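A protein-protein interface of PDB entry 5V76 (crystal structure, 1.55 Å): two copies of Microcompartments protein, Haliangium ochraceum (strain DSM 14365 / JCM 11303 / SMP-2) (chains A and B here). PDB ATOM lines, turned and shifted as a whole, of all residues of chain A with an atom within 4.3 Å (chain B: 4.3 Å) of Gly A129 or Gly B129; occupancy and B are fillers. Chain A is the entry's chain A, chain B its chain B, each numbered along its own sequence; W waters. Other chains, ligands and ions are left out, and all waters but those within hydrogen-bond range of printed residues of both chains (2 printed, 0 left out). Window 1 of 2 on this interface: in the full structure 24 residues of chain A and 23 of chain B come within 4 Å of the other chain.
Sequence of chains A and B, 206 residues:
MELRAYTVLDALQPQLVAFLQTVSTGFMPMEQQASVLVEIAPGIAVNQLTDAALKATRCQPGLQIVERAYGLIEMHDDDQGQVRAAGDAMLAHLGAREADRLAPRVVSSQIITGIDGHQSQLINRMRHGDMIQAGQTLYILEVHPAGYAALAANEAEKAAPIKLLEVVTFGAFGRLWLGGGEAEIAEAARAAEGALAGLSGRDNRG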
ATOM      1  N   PHE A  19      21.101  -6.210  -6.344  1.00  0.00           N
ATOM      2  CA  PHE A  19      20.205  -7.341  -6.564  1.00  0.00           C
ATOM      3  C   PHE A  19      20.056  -7.638  -8.047  1.00  0.00           C
ATOM      4  O   PHE A  19      20.163  -8.791  -8.484  1.00  0.00           O
ATOM      5  CB  PHE A  19      18.837  -7.042  -5.943  1.00  0.00           C
ATOM      6  CG  PHE A  19      17.875  -8.184  -6.042  1.00  0.00           C
ATOM      7  CD1 PHE A  19      17.073  -8.324  -7.154  1.00  0.00           C
ATOM      8  CD2 PHE A  19      17.798  -9.131  -5.030  1.00  0.00           C
ATOM      9  CE1 PHE A  19      16.202  -9.393  -7.261  1.00  0.00           C
ATOM     10  CE2 PHE A  19      16.921 -10.197  -5.141  1.00  0.00           C
ATOM     11  CZ  PHE A  19      16.149 -10.329  -6.252  1.00  0.00           C
ATOM     12  N   ARG A 127      16.202 -16.258  -0.638  1.00  0.00           N
ATOM     13  CA  ARG A 127      16.423 -14.931  -1.197  1.00  0.00           C
ATOM     14  C   ARG A 127      17.695 -14.874  -2.045  1.00  0.00           C
ATOM     15  O   ARG A 127      18.603 -15.715  -1.930  1.00  0.00           O
ATOM     16  CB  ARG A 127      16.487 -13.885  -0.079  1.00  0.00           C
ATOM     17  CG  ARG A 127      17.499 -14.119   1.037  1.00  0.00           C
ATOM     18  CD  ARG A 127      18.954 -13.801   0.656  1.00  0.00           C
ATOM     19  NE  ARG A 127      19.855 -14.794   1.202  1.00  0.00           N
ATOM     20  CZ  ARG A 127      21.178 -14.752   1.143  1.00  0.00           C
ATOM     21  NH1 ARG A 127      21.885 -15.747   1.677  1.00  0.00           N
ATOM     22  NH2 ARG A 127      21.786 -13.754   0.525  1.00  0.00           N
ATOM     23  N   HIS A 128      17.768 -13.825  -2.880  1.00  0.00           N
ATOM     24  CA  HIS A 128      18.966 -13.527  -3.657  1.00  0.00           C
ATOM     25  C   HIS A 128      19.616 -12.197  -3.299  1.00  0.00           C
ATOM     26  O   HIS A 128      20.669 -11.867  -3.866  1.00  0.00           O
ATOM     27  CB  HIS A 128      18.648 -13.528  -5.160  1.00  0.00           C
ATOM     28  CG  HIS A 128      18.038 -14.807  -5.624  1.00  0.00           C
ATOM     29  ND1 HIS A 128      16.682 -15.036  -5.578  1.00  0.00           N
ATOM     30  CD2 HIS A 128      18.599 -15.944  -6.101  1.00  0.00           C
ATOM     31  CE1 HIS A 128      16.426 -16.253  -6.022  1.00  0.00           C
ATOM     32  NE2 HIS A 128      17.571 -16.828  -6.344  1.00  0.00           N
ATOM     33  N   GLY A 129      19.010 -11.407  -2.412  1.00  0.00           N
ATOM     34  CA  GLY A 129      19.581 -10.157  -1.946  1.00  0.00           C
ATOM     35  C   GLY A 129      20.371 -10.308  -0.665  1.00  0.00           C
ATOM     36  O   GLY A 129      21.182 -11.232  -0.540  1.00  0.00           O
ATOM     37  N   ASP A 130      20.167  -9.380   0.271  1.00  0.00           N
ATOM     38  CA  ASP A 130      20.831  -9.444   1.568  1.00  0.00           C
ATOM     39  C   ASP A 130      20.190 -10.513   2.456  1.00  0.00           C
ATOM     40  O   ASP A 130      19.069 -10.988   2.212  1.00  0.00           O
ATOM     41  CB  ASP A 130      20.746  -8.103   2.309  1.00  0.00           C
ATOM     42  CG  ASP A 130      21.925  -7.169   2.030  1.00  0.00           C
ATOM     43  OD1 ASP A 130      22.879  -7.543   1.325  1.00  0.00           O
ATOM     44  OD2 ASP A 130      21.887  -6.040   2.546  1.00  0.00           O
ATOM     45  N   MET A 131      20.909 -10.853   3.522  1.00  0.00           N
ATOM     46  CA  MET A 131      20.432 -11.798   4.522  1.00  0.00           C
ATOM     47  C   MET A 131      19.657 -11.085   5.622  1.00  0.00           C
ATOM     48  O   MET A 131      19.771  -9.878   5.809  1.00  0.00           O
ATOM     49  CB  MET A 131      21.599 -12.545   5.150  1.00  0.00           C
ATOM     50  CG  MET A 131      22.508 -13.217   4.131  1.00  0.00           C
ATOM     51  SD  MET A 131      23.843 -14.254   4.783  1.00  0.00           S
ATOM     52  CE  MET A 131      24.914 -13.056   5.551  1.00  0.00           C
ATOM     53  N   LEU A 164      17.237  -5.023   1.241  1.00  0.00           N
ATOM     54  CA  LEU A 164      16.490  -5.678   0.175  1.00  0.00           C
ATOM     55  C   LEU A 164      16.823  -7.169   0.188  1.00  0.00           C
ATOM     56  O   LEU A 164      17.952  -7.566  -0.112  1.00  0.00           O
ATOM     57  CB  LEU A 164      16.825  -5.062  -1.182  1.00  0.00           C
ATOM     58  CG  LEU A 164      16.179  -5.758  -2.389  1.00  0.00           C
ATOM     59  CD1 LEU A 164      14.688  -5.768  -2.297  1.00  0.00           C
ATOM     60  CD2 LEU A 164      16.616  -5.084  -3.682  1.00  0.00           C
ATOM     61  N   LEU A 165      15.839  -7.996   0.547  1.00  0.00           N
ATOM     62  CA  LEU A 165      16.065  -9.440   0.620  1.00  0.00           C
ATOM     63  C   LEU A 165      15.759 -10.129  -0.710  1.00  0.00           C
ATOM     64  O   LEU A 165      16.538 -10.954  -1.201  1.00  0.00           O
ATOM     65  CB  LEU A 165      15.200 -10.033   1.737  1.00  0.00           C
ATOM     66  CG  LEU A 165      15.268  -9.293   3.062  1.00  0.00           C
ATOM     67  CD1 LEU A 165      14.337  -9.986   4.062  1.00  0.00           C
ATOM     68  CD2 LEU A 165      16.684  -9.209   3.587  1.00  0.00           C
ATOM     69  N   PHE B  19      24.497 -17.265   6.640  1.00  0.00           N
ATOM     70  CA  PHE B  19      25.206 -17.832   5.499  1.00  0.00           C
ATOM     71  C   PHE B  19      25.139 -19.348   5.511  1.00  0.00           C
ATOM     72  O   PHE B  19      24.816 -19.981   4.503  1.00  0.00           O
ATOM     73  CB  PHE B  19      26.665 -17.363   5.507  1.00  0.00           C
ATOM     74  CG  PHE B  19      27.434 -17.818   4.309  1.00  0.00           C
ATOM     75  CD1 PHE B  19      28.046 -19.052   4.284  1.00  0.00           C
ATOM     76  CD2 PHE B  19      27.503 -17.018   3.172  1.00  0.00           C
ATOM     77  CE1 PHE B  19      28.736 -19.484   3.165  1.00  0.00           C
ATOM     78  CE2 PHE B  19      28.194 -17.459   2.049  1.00  0.00           C
ATOM     79  CZ  PHE B  19      28.792 -18.683   2.043  1.00  0.00           C
ATOM     80  N   ARG B 127      28.567 -14.307  -4.845  1.00  0.00           N
ATOM     81  CA  ARG B 127      28.477 -14.570  -3.411  1.00  0.00           C
ATOM     82  C   ARG B 127      27.140 -15.199  -3.024  1.00  0.00           C
ATOM     83  O   ARG B 127      26.152 -15.157  -3.768  1.00  0.00           O
ATOM     84  CB  ARG B 127      28.678 -13.275  -2.618  1.00  0.00           C
ATOM     85  CG  ARG B 127      27.745 -12.116  -2.976  1.00  0.00           C
ATOM     86  CD  ARG B 127      26.307 -12.219  -2.430  1.00  0.00           C
ATOM     87  NE  ARG B 127      25.356 -11.736  -3.415  1.00  0.00           N
ATOM     88  CZ  ARG B 127      24.062 -11.579  -3.203  1.00  0.00           C
ATOM     89  NH1 ARG B 127      23.277 -11.165  -4.183  1.00  0.00           N
ATOM     90  NH2 ARG B 127      23.530 -11.879  -2.039  1.00  0.00           N
ATOM     91  N   HIS B 128      27.117 -15.783  -1.820  1.00  0.00           N
ATOM     92  CA  HIS B 128      25.890 -16.311  -1.239  1.00  0.00           C
ATOM     93  C   HIS B 128      25.489 -15.619   0.047  1.00  0.00           C
ATOM     94  O   HIS B 128      24.427 -15.941   0.595  1.00  0.00           O
ATOM     95  CB  HIS B 128      26.034 -17.822  -0.991  1.00  0.00           C
ATOM     96  CG  HIS B 128      26.352 -18.595  -2.226  1.00  0.00           C
ATOM     97  ND1 HIS B 128      27.642 -18.818  -2.650  1.00  0.00           N
ATOM     98  CD2 HIS B 128      25.545 -19.149  -3.163  1.00  0.00           C
ATOM     99  CE1 HIS B 128      27.620 -19.492  -3.790  1.00  0.00           C
ATOM    100  NE2 HIS B 128      26.358 -19.705  -4.122  1.00  0.00           N
ATOM    101  N   GLY B 129      26.294 -14.691   0.551  1.00  0.00           N
ATOM    102  CA  GLY B 129      25.955 -13.939   1.744  1.00  0.00           C
ATOM    103  C   GLY B 129      25.341 -12.595   1.430  1.00  0.00           C
ATOM    104  O   GLY B 129      24.447 -12.511   0.584  1.00  0.00           O
ATOM    105  N   ASP B 130      25.794 -11.538   2.102  1.00  0.00           N
ATOM    106  CA  ASP B 130      25.272 -10.199   1.875  1.00  0.00           C
ATOM    107  C   ASP B 130      25.832  -9.629   0.581  1.00  0.00           C
ATOM    108  O   ASP B 130      26.827 -10.118   0.038  1.00  0.00           O
ATOM    109  CB  ASP B 130      25.654  -9.255   3.014  1.00  0.00           C
ATOM    110  CG  ASP B 130      24.576  -9.125   4.077  1.00  0.00           C
ATOM    111  OD1 ASP B 130      23.540  -9.826   4.027  1.00  0.00           O
ATOM    112  OD2 ASP B 130      24.781  -8.288   4.983  1.00  0.00           O
ATOM    113  N   MET B 131      25.192  -8.564   0.106  1.00  0.00           N
ATOM    114  CA  MET B 131      25.641  -7.869  -1.098  1.00  0.00           C
ATOM    115  C   MET B 131      26.651  -6.784  -0.725  1.00  0.00           C
ATOM    116  O   MET B 131      26.748  -6.375   0.431  1.00  0.00           O
ATOM    117  CB  MET B 131      24.457  -7.245  -1.840  1.00  0.00           C
ATOM    118  CG  MET B 131      23.342  -8.252  -2.135  1.00  0.00           C
ATOM    119  SD  MET B 131      22.038  -7.577  -3.142  1.00  0.00           S
ATOM    120  CE  MET B 131      21.262  -6.442  -2.007  1.00  0.00           C
ATOM    121  N   LEU B 164      29.441 -10.243   5.787  1.00  0.00           N
ATOM    122  CA  LEU B 164      29.946 -11.518   5.291  1.00  0.00           C
ATOM    123  C   LEU B 164      29.392 -11.709   3.894  1.00  0.00           C
ATOM    124  O   LEU B 164      28.175 -11.845   3.726  1.00  0.00           O
ATOM    125  CB  LEU B 164      29.529 -12.673   6.200  1.00  0.00           C
ATOM    126  CG  LEU B 164      29.868 -14.062   5.690  1.00  0.00           C
ATOM    127  CD1 LEU B 164      31.362 -14.225   5.501  1.00  0.00           C
ATOM    128  CD2 LEU B 164      29.322 -15.104   6.658  1.00  0.00           C
ATOM    129  N   LEU B 165      30.270 -11.664   2.897  1.00  0.00           N
ATOM    130  CA  LEU B 165      29.845 -11.821   1.508  1.00  0.00           C
ATOM    131  C   LEU B 165      29.894 -13.284   1.095  1.00  0.00           C
ATOM    132  O   LEU B 165      28.927 -13.818   0.543  1.00  0.00           O
ATOM    133  CB  LEU B 165      30.728 -10.979   0.574  1.00  0.00           C
ATOM    134  CG  LEU B 165      30.949  -9.542   1.018  1.00  0.00           C
ATOM    135  CD1 LEU B 165      31.895  -8.897   0.001  1.00  0.00           C
ATOM    136  CD2 LEU B 165      29.656  -8.767   1.162  1.00  0.00           C
HETATM  137  O   HOH W   1      24.031  -4.838   1.123  1.00  0.00           O
HETATM  138  O   HOH W   2      22.656  -9.386   6.693  1.00  0.00           O
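N of Met B131 is in hydrogen-bond range of OD1 of Asp A130, 2.8 Å away. The backbone NH (N) of Phe B19 lies within hydrogen-bond range of the side-chain sulfur (SD) of Met A131 (3.6 Å). The guanidinium group (NH2) of Arg A127 sits at hydrogen-bond distance from the backbone carbonyl oxygen (O) of Gly B129 (2.9 Å). O of His B128 sits at hydrogen-bond distance from NH1 of Arg A127, 2.8 Å away. N of Met A131 is in hydrogen-bond range of OD1 of Asp B130, 2.9 Å away. The backbone carbonyl oxygen of His A128 lies within hydrogen-bond range of the guanidinium group of Arg B127 (2.7 Å). The backbone NH of Phe A19 sits at hydrogen-bond distance from the side-chain sulfur of Met B131, at 3.6 Å. The guanidinium group (NH2) of Arg B127 sits at hydrogen-bond distance from the backbone carbonyl oxygen (O) of Gly A129 (2.9 Å).
Water W1 lies within hydrogen-bond range of OD2 of Asp A130 (2.8 Å) and O of Met B131 (3.2 Å). Water W2 lies within hydrogen-bond range of OD1 of Asp B130 and O of Met A131.
Phe A19 touches Met B131, and with the chains exchanged Met A131 touches Phe B19. Arg A127 touches His B128, and with the chains exchanged His A128 touches Arg B127. Asp A130 touches Met B131, and with the chains exchanged Met A131 touches Asp B130. Met A131 touches Leu B164, and with the chains exchanged Leu A164 touches Met B131. Positions printed for both chains: 19, 127, 128, 129, 130, 131, 164 and 165. Of the 15 pairs that touch across the chains among the printed residues, 15 have their exchanged pair printed and touching as well.
The backbone carbonyl oxygen (O) of Gly A129 sits at hydrogen-bond distance from the guanidinium group (NH2) of Arg A127, 2.8 Å away. The backbone carbonyl oxygen (O) of Leu A165 lies within hydrogen-bond range of the backbone NH (N) of Gly A129 (2.8 Å). The backbone NH of Asp A130 sits at hydrogen-bond distance from the backbone carbonyl oxygen of Leu A164 (2.9 Å). The backbone NH of Gly B129 sits at hydrogen-bond distance from the backbone carbonyl oxygen of Leu B165. The backbone NH (N) of Asp B130 sits at hydrogen-bond distance from the backbone carbonyl oxygen (O) of Leu B164, 2.9 Å away. NH2 of Arg B127 sits at hydrogen-bond distance from O of Gly B129 (2.8 Å).
NH2 of Arg B127 touches NH2 of Arg A127, at 3.6 Å. O of Gly A129 touches O of Gly B129, at 3.7 Å. SD of Met B131 touches CA of Gly A129, 3.8 Å away. OD1 of Asp A130 touches OD1 of Asp B130 (3.6 Å). Met A131 touches Gly B129 (SD to CA, 3.7 Å). O of Leu B164 touches CE of Met A131, at 3.9 Å. O of Leu A164 touches CE of Met B131 (3.98 Å).
Printed residues of chain B within 4 Å of Arg A127: Arg B127, His B128 and Gly B129. Printed residues of chain B within 4 Å of Gly A129: Arg B127 (2.9 Å), Gly B129 (3.7 Å) and Met B131 (3.8 Å). Leu A165 touches none of the printed residues of chain B. Of the printed residues of chain A, Phe B19 touches Met A131. Gly B129 touches three residues of chain A. The nearest printed residue of chain B that does not touch Gly A129 is Asp B130 (4.9 Å). The nearest printed residue of chain A that does not touch Asp B130 is Arg A127 (4.8 Å).
Hydrophobic or aromatic side chains of chain B that line the printed part of chain A: Met B131. Printed residues of chain A that touch a printed residue of chain B: Phe A19, Arg A127, His A128, Gly A129, Asp A130, Met A131 and Leu A164. Hydrophobic or aromatic side chains of chain A that line the printed part of chain B: Met A131. Among the printed residues, 15 pairs touch across the chains. Among the printed residues, no Asp or Glu carboxylate lies within 4 Å of a Lys or Arg side-chain nitrogen of the other chain.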
